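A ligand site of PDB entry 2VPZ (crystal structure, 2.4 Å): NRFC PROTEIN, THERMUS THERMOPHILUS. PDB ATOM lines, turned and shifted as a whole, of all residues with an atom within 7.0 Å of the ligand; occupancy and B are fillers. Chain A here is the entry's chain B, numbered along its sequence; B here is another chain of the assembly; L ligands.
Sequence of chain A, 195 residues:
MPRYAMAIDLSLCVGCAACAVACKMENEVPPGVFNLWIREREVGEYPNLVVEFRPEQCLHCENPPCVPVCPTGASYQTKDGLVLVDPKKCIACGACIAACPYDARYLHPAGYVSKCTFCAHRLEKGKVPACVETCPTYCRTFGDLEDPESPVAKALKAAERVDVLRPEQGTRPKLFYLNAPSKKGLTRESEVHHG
The backbone NH of Cys 19 lies close to a sulfur (S2) of the ligand, 3.3 Å away.
An iron atom (FE4) of the ligand is bound by the side-chain sulfur (SG) of Cys 19 (2.2 Å).
An iron atom (FE2) of the ligand is bound by the side-chain sulfur (SG) of Cys 13 (2.3 Å).
O of Cys 16 binds FE3 of the ligand.
The side-chain sulfur of Cys 16 binds an iron atom (FE3) of the ligand (2.4 Å).
The side-chain sulfur (SG) of Cys 135 binds an iron atom (FE1) of the ligand (2.5 Å).
A sulfur (S3) of the ligand sits close to the side-chain sulfur (SG) of Cys 139.
N of Val 14 lies close to S4 of the ligand, at 3.7 Å.
The side-chain sulfur (SG) of Cys 19 sits close to the guanidinium group (NH1) of Arg 140, 3.4 Å away.
SG of Cys 16 lies close to N of Ala 18 (3.8 Å).
The side-chain sulfur of Cys 135 sits close to the side-chain hydroxyl of Thr 137.
The side-chain sulfur of Cys 139 is in hydrogen-bond range of the side-chain hydroxyl of Thr 137.
The backbone NH of Asp 9 sits at hydrogen-bond distance from the backbone carbonyl oxygen of Cys 139, 2.9 Å away.
The guanidinium group of Arg 140 lies close to the side-chain sulfur of Cys 131 (3.6 Å).
Residues that only touch the ligand: Ile 38 (3.2 Å), Ala 18 (3.6 Å), Arg 140 (3.7 Å) and Thr 137 (3.8 Å).
Hydrophobic or aromatic side chains that line the ligand: Ala 18 and Ile 38.
Of the 28 residues printed, 10 come within 4 Å of the ligand.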
ATOM      1  N   ILE A   8      18.812  11.429   1.934  1.00  0.00           N
ATOM      2  CA  ILE A   8      17.636  10.875   1.301  1.00  0.00           C
ATOM      3  C   ILE A   8      16.498  11.877   1.373  1.00  0.00           C
ATOM      4  O   ILE A   8      16.148  12.414   2.438  1.00  0.00           O
ATOM      5  CB  ILE A   8      17.152   9.536   1.972  1.00  0.00           C
ATOM      6  CG1 ILE A   8      18.322   8.559   2.174  1.00  0.00           C
ATOM      7  CG2 ILE A   8      16.038   8.885   1.095  1.00  0.00           C
ATOM      8  CD1 ILE A   8      17.908   7.125   2.586  1.00  0.00           C
ATOM      9  N   ASP A   9      15.929  12.161   0.201  1.00  0.00           N
ATOM     10  CA  ASP A   9      14.793  13.089   0.038  1.00  0.00           C
ATOM     11  C   ASP A   9      13.548  12.233   0.285  1.00  0.00           C
ATOM     12  O   ASP A   9      13.296  11.248  -0.427  1.00  0.00           O
ATOM     13  CB  ASP A   9      14.822  13.666  -1.383  1.00  0.00           C
ATOM     14  CG  ASP A   9      13.953  14.927  -1.548  1.00  0.00           C
ATOM     15  OD1 ASP A   9      13.076  15.161  -0.708  1.00  0.00           O
ATOM     16  OD2 ASP A   9      14.154  15.648  -2.561  1.00  0.00           O
ATOM     17  N   LEU A  12      10.418  12.586  -2.271  1.00  0.00           N
ATOM     18  CA  LEU A  12      10.521  11.796  -3.503  1.00  0.00           C
ATOM     19  C   LEU A  12      10.467  10.263  -3.278  1.00  0.00           C
ATOM     20  O   LEU A  12      10.053   9.528  -4.184  1.00  0.00           O
ATOM     21  CB  LEU A  12      11.832  12.124  -4.265  1.00  0.00           C
ATOM     22  CG  LEU A  12      12.185  13.557  -4.662  1.00  0.00           C
ATOM     23  CD1 LEU A  12      13.572  13.524  -5.279  1.00  0.00           C
ATOM     24  CD2 LEU A  12      11.191  14.175  -5.669  1.00  0.00           C
ATOM     25  N   CYS A  13      10.878   9.788  -2.108  1.00  0.00           N
ATOM     26  CA  CYS A  13      10.879   8.353  -1.785  1.00  0.00           C
ATOM     27  C   CYS A  13       9.472   7.692  -1.861  1.00  0.00           C
ATOM     28  O   CYS A  13       8.500   8.201  -1.284  1.00  0.00           O
ATOM     29  CB  CYS A  13      11.554   8.062  -0.421  1.00  0.00           C
ATOM     30  SG  CYS A  13      12.042   6.254  -0.228  1.00  0.00           S
ATOM     31  N   VAL A  14       9.342   6.577  -2.567  1.00  0.00           N
ATOM     32  CA  VAL A  14       8.041   5.925  -2.702  1.00  0.00           C
ATOM     33  C   VAL A  14       7.967   4.535  -2.061  1.00  0.00           C
ATOM     34  O   VAL A  14       6.952   3.847  -2.166  1.00  0.00           O
ATOM     35  CB  VAL A  14       7.517   5.914  -4.198  1.00  0.00           C
ATOM     36  CG1 VAL A  14       7.551   7.355  -4.769  1.00  0.00           C
ATOM     37  CG2 VAL A  14       8.319   4.944  -5.064  1.00  0.00           C
ATOM     38  N   GLY A  15       9.041   4.159  -1.377  1.00  0.00           N
ATOM     39  CA  GLY A  15       9.159   2.894  -0.666  1.00  0.00           C
ATOM     40  C   GLY A  15       9.084   1.591  -1.449  1.00  0.00           C
ATOM     41  O   GLY A  15       8.524   0.606  -0.943  1.00  0.00           O
ATOM     42  N   CYS A  16       9.619   1.581  -2.671  1.00  0.00           N
ATOM     43  CA  CYS A  16       9.706   0.423  -3.601  1.00  0.00           C
ATOM     44  C   CYS A  16      11.035  -0.142  -3.094  1.00  0.00           C
ATOM     45  O   CYS A  16      12.060   0.378  -3.452  1.00  0.00           O
ATOM     46  CB  CYS A  16       9.922   0.953  -5.028  1.00  0.00           C
ATOM     47  SG  CYS A  16      11.631   1.958  -5.123  1.00  0.00           S
ATOM     48  N   ALA A  17      11.119  -1.190  -2.303  1.00  0.00           N
ATOM     49  CA  ALA A  17      12.491  -1.462  -1.814  1.00  0.00           C
ATOM     50  C   ALA A  17      13.659  -1.715  -2.831  1.00  0.00           C
ATOM     51  O   ALA A  17      14.451  -2.622  -2.625  1.00  0.00           O
ATOM     52  CB  ALA A  17      12.445  -2.595  -0.745  1.00  0.00           C
ATOM     53  N   ALA A  18      13.834  -0.876  -3.878  1.00  0.00           N
ATOM     54  CA  ALA A  18      14.880  -1.172  -4.877  1.00  0.00           C
ATOM     55  C   ALA A  18      16.312  -1.223  -4.322  1.00  0.00           C
ATOM     56  O   ALA A  18      17.091  -2.148  -4.600  1.00  0.00           O
ATOM     57  CB  ALA A  18      14.813  -0.208  -6.098  1.00  0.00           C
ATOM     58  N   CYS A  19      16.605  -0.220  -3.509  1.00  0.00           N
ATOM     59  CA  CYS A  19      17.846  -0.022  -2.779  1.00  0.00           C
ATOM     60  C   CYS A  19      18.072  -1.220  -1.835  1.00  0.00           C
ATOM     61  O   CYS A  19      19.179  -1.773  -1.767  1.00  0.00           O
ATOM     62  CB  CYS A  19      17.780   1.298  -1.969  1.00  0.00           C
ATOM     63  SG  CYS A  19      16.346   1.490  -0.804  1.00  0.00           S
ATOM     64  N   ALA A  20      17.030  -1.632  -1.125  1.00  0.00           N
ATOM     65  CA  ALA A  20      17.125  -2.770  -0.192  1.00  0.00           C
ATOM     66  C   ALA A  20      17.478  -4.099  -0.901  1.00  0.00           C
ATOM     67  O   ALA A  20      18.280  -4.894  -0.370  1.00  0.00           O
ATOM     68  CB  ALA A  20      15.812  -2.907   0.653  1.00  0.00           C
ATOM     69  N   LEU A  36      19.712  -2.941   5.207  1.00  0.00           N
ATOM     70  CA  LEU A  36      18.763  -1.878   4.757  1.00  0.00           C
ATOM     71  C   LEU A  36      17.319  -2.409   4.663  1.00  0.00           C
ATOM     72  O   LEU A  36      17.124  -3.524   4.166  1.00  0.00           O
ATOM     73  CB  LEU A  36      19.199  -1.354   3.348  1.00  0.00           C
ATOM     74  CG  LEU A  36      18.387  -0.398   2.430  1.00  0.00           C
ATOM     75  CD1 LEU A  36      17.775   0.676   3.303  1.00  0.00           C
ATOM     76  CD2 LEU A  36      19.245   0.264   1.300  1.00  0.00           C
ATOM     77  N   TRP A  37      16.343  -1.651   5.158  1.00  0.00           N
ATOM     78  CA  TRP A  37      14.914  -2.007   5.152  1.00  0.00           C
ATOM     79  C   TRP A  37      14.156  -0.693   4.999  1.00  0.00           C
ATOM     80  O   TRP A  37      14.748   0.377   5.181  1.00  0.00           O
ATOM     81  CB  TRP A  37      14.465  -2.690   6.458  1.00  0.00           C
ATOM     82  CG  TRP A  37      14.769  -1.902   7.752  1.00  0.00           C
ATOM     83  CD1 TRP A  37      13.900  -1.100   8.488  1.00  0.00           C
ATOM     84  CD2 TRP A  37      16.019  -1.888   8.462  1.00  0.00           C
ATOM     85  NE1 TRP A  37      14.558  -0.602   9.606  1.00  0.00           N
ATOM     86  CE2 TRP A  37      15.848  -1.066   9.610  1.00  0.00           C
ATOM     87  CE3 TRP A  37      17.256  -2.482   8.233  1.00  0.00           C
ATOM     88  CZ2 TRP A  37      16.892  -0.831  10.533  1.00  0.00           C
ATOM     89  CZ3 TRP A  37      18.305  -2.267   9.148  1.00  0.00           C
ATOM     90  CH2 TRP A  37      18.109  -1.439  10.285  1.00  0.00           C
ATOM     91  N   ILE A  38      12.872  -0.771   4.688  1.00  0.00           N
ATOM     92  CA  ILE A  38      12.019   0.406   4.508  1.00  0.00           C
ATOM     93  C   ILE A  38      10.877   0.353   5.542  1.00  0.00           C
ATOM     94  O   ILE A  38      10.239  -0.684   5.695  1.00  0.00           O
ATOM     95  CB  ILE A  38      11.283   0.417   3.079  1.00  0.00           C
ATOM     96  CG1 ILE A  38      12.237   0.018   1.938  1.00  0.00           C
ATOM     97  CG2 ILE A  38      10.536   1.781   2.895  1.00  0.00           C
ATOM     98  CD1 ILE A  38      13.435   0.911   1.677  1.00  0.00           C
ATOM     99  N   PHE A  53       7.461   7.175   3.931  1.00  0.00           N
ATOM    100  CA  PHE A  53       8.221   6.027   3.431  1.00  0.00           C
ATOM    101  C   PHE A  53       9.654   6.308   3.924  1.00  0.00           C
ATOM    102  O   PHE A  53      10.201   7.357   3.620  1.00  0.00           O
ATOM    103  CB  PHE A  53       8.165   5.986   1.910  1.00  0.00           C
ATOM    104  CG  PHE A  53       6.770   5.961   1.351  1.00  0.00           C
ATOM    105  CD1 PHE A  53       6.167   7.123   0.870  1.00  0.00           C
ATOM    106  CD2 PHE A  53       6.075   4.753   1.293  1.00  0.00           C
ATOM    107  CE1 PHE A  53       4.862   7.098   0.340  1.00  0.00           C
ATOM    108  CE2 PHE A  53       4.774   4.691   0.770  1.00  0.00           C
ATOM    109  CZ  PHE A  53       4.156   5.864   0.292  1.00  0.00           C
ATOM    110  N   ARG A  54      10.302   5.393   4.637  1.00  0.00           N
ATOM    111  CA  ARG A  54      11.610   5.725   5.198  1.00  0.00           C
ATOM    112  C   ARG A  54      12.666   4.641   5.175  1.00  0.00           C
ATOM    113  O   ARG A  54      12.514   3.663   5.913  1.00  0.00           O
ATOM    114  CB  ARG A  54      11.346   6.182   6.644  1.00  0.00           C
ATOM    115  CG  ARG A  54      12.333   7.102   7.314  1.00  0.00           C
ATOM    116  CD  ARG A  54      12.513   6.612   8.761  1.00  0.00           C
ATOM    117  NE  ARG A  54      11.746   7.421   9.689  1.00  0.00           N
ATOM    118  CZ  ARG A  54      11.327   7.067  10.900  1.00  0.00           C
ATOM    119  NH1 ARG A  54      11.573   5.891  11.397  1.00  0.00           N
ATOM    120  NH2 ARG A  54      10.621   7.942  11.611  1.00  0.00           N
ATOM    121  N   PRO A  55      13.713   4.737   4.319  1.00  0.00           N
ATOM    122  CA  PRO A  55      14.684   3.635   4.395  1.00  0.00           C
ATOM    123  C   PRO A  55      15.548   3.779   5.688  1.00  0.00           C
ATOM    124  O   PRO A  55      15.883   4.895   6.057  1.00  0.00           O
ATOM    125  CB  PRO A  55      15.526   3.757   3.104  1.00  0.00           C
ATOM    126  CG  PRO A  55      14.949   4.918   2.298  1.00  0.00           C
ATOM    127  CD  PRO A  55      13.986   5.673   3.228  1.00  0.00           C
ATOM    128  N   CYS A 131      23.025   1.028  -3.355  1.00  0.00           N
ATOM    129  CA  CYS A 131      21.716   1.679  -3.109  1.00  0.00           C
ATOM    130  C   CYS A 131      21.551   2.969  -3.935  1.00  0.00           C
ATOM    131  O   CYS A 131      20.474   3.227  -4.496  1.00  0.00           O
ATOM    132  CB  CYS A 131      21.479   2.076  -1.630  1.00  0.00           C
ATOM    133  SG  CYS A 131      22.923   2.483  -0.562  1.00  0.00           S
ATOM    134  N   THR A 134      21.240   2.157  -8.222  1.00  0.00           N
ATOM    135  CA  THR A 134      19.866   1.613  -8.512  1.00  0.00           C
ATOM    136  C   THR A 134      18.819   2.379  -7.692  1.00  0.00           C
ATOM    137  O   THR A 134      18.593   2.072  -6.517  1.00  0.00           O
ATOM    138  CB  THR A 134      19.568   0.136  -8.066  1.00  0.00           C
ATOM    139  OG1 THR A 134      18.579  -0.457  -8.905  1.00  0.00           O
ATOM    140  CG2 THR A 134      18.999   0.133  -6.603  1.00  0.00           C
ATOM    141  N   CYS A 135      18.174   3.374  -8.271  1.00  0.00           N
ATOM    142  CA  CYS A 135      17.154   4.162  -7.577  1.00  0.00           C
ATOM    143  C   CYS A 135      16.417   4.982  -8.604  1.00  0.00           C
ATOM    144  O   CYS A 135      16.867   6.055  -9.059  1.00  0.00           O
ATOM    145  CB  CYS A 135      17.698   5.070  -6.463  1.00  0.00           C
ATOM    146  SG  CYS A 135      16.266   6.008  -5.375  1.00  0.00           S
ATOM    147  N   PRO A 136      15.254   4.462  -9.004  1.00  0.00           N
ATOM    148  CA  PRO A 136      14.364   5.070  -9.984  1.00  0.00           C
ATOM    149  C   PRO A 136      14.055   6.548  -9.698  1.00  0.00           C
ATOM    150  O   PRO A 136      14.115   7.388 -10.585  1.00  0.00           O
ATOM    151  CB  PRO A 136      13.102   4.208  -9.928  1.00  0.00           C
ATOM    152  CG  PRO A 136      13.462   2.957  -9.146  1.00  0.00           C
ATOM    153  CD  PRO A 136      14.616   3.374  -8.264  1.00  0.00           C
ATOM    154  N   THR A 137      13.758   6.865  -8.444  1.00  0.00           N
ATOM    155  CA  THR A 137      13.374   8.232  -8.067  1.00  0.00           C
ATOM    156  C   THR A 137      14.457   9.315  -7.864  1.00  0.00           C
ATOM    157  O   THR A 137      14.147  10.516  -7.802  1.00  0.00           O
ATOM    158  CB  THR A 137      12.465   8.199  -6.789  1.00  0.00           C
ATOM    159  OG1 THR A 137      13.263   7.987  -5.631  1.00  0.00           O
ATOM    160  CG2 THR A 137      11.428   7.061  -6.891  1.00  0.00           C
ATOM    161  N   TYR A 138      15.721   8.892  -7.793  1.00  0.00           N
ATOM    162  CA  TYR A 138      16.884   9.770  -7.548  1.00  0.00           C
ATOM    163  C   TYR A 138      16.761  10.541  -6.206  1.00  0.00           C
ATOM    164  O   TYR A 138      17.092  11.719  -6.145  1.00  0.00           O
ATOM    165  CB  TYR A 138      17.112  10.781  -8.692  1.00  0.00           C
ATOM    166  CG  TYR A 138      17.148  10.222 -10.110  1.00  0.00           C
ATOM    167  CD1 TYR A 138      15.964  10.097 -10.857  1.00  0.00           C
ATOM    168  CD2 TYR A 138      18.343   9.775 -10.693  1.00  0.00           C
ATOM    169  CE1 TYR A 138      15.966   9.529 -12.163  1.00  0.00           C
ATOM    170  CE2 TYR A 138      18.353   9.218 -11.994  1.00  0.00           C
ATOM    171  CZ  TYR A 138      17.173   9.086 -12.733  1.00  0.00           C
ATOM    172  OH  TYR A 138      17.209   8.529 -14.002  1.00  0.00           O
ATOM    173  N   CYS A 139      16.271   9.898  -5.152  1.00  0.00           N
ATOM    174  CA  CYS A 139      16.150  10.606  -3.873  1.00  0.00           C
ATOM    175  C   CYS A 139      17.385  10.480  -2.952  1.00  0.00           C
ATOM    176  O   CYS A 139      17.503  11.275  -2.017  1.00  0.00           O
ATOM    177  CB  CYS A 139      14.876  10.201  -3.115  1.00  0.00           C
ATOM    178  SG  CYS A 139      14.940   8.522  -2.454  1.00  0.00           S
ATOM    179  N   ARG A 140      18.272   9.486  -3.173  1.00  0.00           N
ATOM    180  CA  ARG A 140      19.510   9.396  -2.367  1.00  0.00           C
ATOM    181  C   ARG A 140      20.759  10.042  -3.010  1.00  0.00           C
ATOM    182  O   ARG A 140      20.979   9.989  -4.221  1.00  0.00           O
ATOM    183  CB  ARG A 140      19.871   7.967  -1.846  1.00  0.00           C
ATOM    184  CG  ARG A 140      19.799   6.753  -2.753  1.00  0.00           C
ATOM    185  CD  ARG A 140      19.060   5.635  -1.976  1.00  0.00           C
ATOM    186  NE  ARG A 140      19.867   5.240  -0.837  1.00  0.00           N
ATOM    187  CZ  ARG A 140      19.472   4.540   0.219  1.00  0.00           C
ATOM    188  NH1 ARG A 140      18.222   4.122   0.330  1.00  0.00           N
ATOM    189  NH2 ARG A 140      20.345   4.279   1.188  1.00  0.00           N
ATOM    190  N   LEU B  78      17.327   0.603 -11.840  1.00  0.00           N
ATOM    191  CA  LEU B  78      16.586  -0.661 -11.840  1.00  0.00           C
ATOM    192  C   LEU B  78      15.617  -0.704 -10.632  1.00  0.00           C
ATOM    193  O   LEU B  78      15.943  -0.217  -9.537  1.00  0.00           O
ATOM    194  CB  LEU B  78      17.580  -1.860 -11.766  1.00  0.00           C
ATOM    195  CG  LEU B  78      17.477  -3.053 -12.754  1.00  0.00           C
ATOM    196  CD1 LEU B  78      17.345  -2.523 -14.216  1.00  0.00           C
ATOM    197  CD2 LEU B  78      18.707  -3.991 -12.634  1.00  0.00           C
ATOM    198  N   PRO B  80      13.147  -2.882  -7.777  1.00  0.00           N
ATOM    199  CA  PRO B  80      13.395  -4.062  -6.929  1.00  0.00           C
ATOM    200  C   PRO B  80      13.261  -5.440  -7.638  1.00  0.00           C
ATOM    201  O   PRO B  80      14.083  -6.351  -7.465  1.00  0.00           O
ATOM    202  CB  PRO B  80      12.430  -3.886  -5.747  1.00  0.00           C
ATOM    203  CG  PRO B  80      11.317  -2.988  -6.320  1.00  0.00           C
ATOM    204  CD  PRO B  80      12.025  -2.070  -7.275  1.00  0.00           C
ATOM    205  N   LEU B 219       8.646   5.424 -13.340  1.00  0.00           N
ATOM    206  CA  LEU B 219       8.861   5.787 -11.926  1.00  0.00           C
ATOM    207  C   LEU B 219       9.860   6.992 -11.992  1.00  0.00           C
ATOM    208  O   LEU B 219       9.620   8.065 -11.424  1.00  0.00           O
ATOM    209  CB  LEU B 219       9.460   4.633 -11.109  1.00  0.00           C
ATOM    210  CG  LEU B 219       9.482   4.774  -9.578  1.00  0.00           C
ATOM    211  CD1 LEU B 219       8.176   5.432  -9.090  1.00  0.00           C
ATOM    212  CD2 LEU B 219       9.712   3.385  -8.910  1.00  0.00           C
HETATM  213 FE1  LIG L   1      14.574   4.929  -3.866  1.00  0.00          FE
HETATM  214 FE2  LIG L   1      13.021   4.712  -1.619  1.00  0.00          FE
HETATM  215 FE3  LIG L   1      13.175   2.649  -3.445  1.00  0.00          FE
HETATM  216 FE4  LIG L   1      15.305   3.201  -1.822  1.00  0.00          FE
HETATM  217  S1  LIG L   1      13.249   2.466  -1.130  1.00  0.00           S
HETATM  218  S2  LIG L   1      15.356   2.767  -4.117  1.00  0.00           S
HETATM  219  S3  LIG L   1      15.168   5.494  -1.675  1.00  0.00           S
HETATM  220  S4  LIG L   1      12.283   4.756  -3.827  1.00  0.00           S
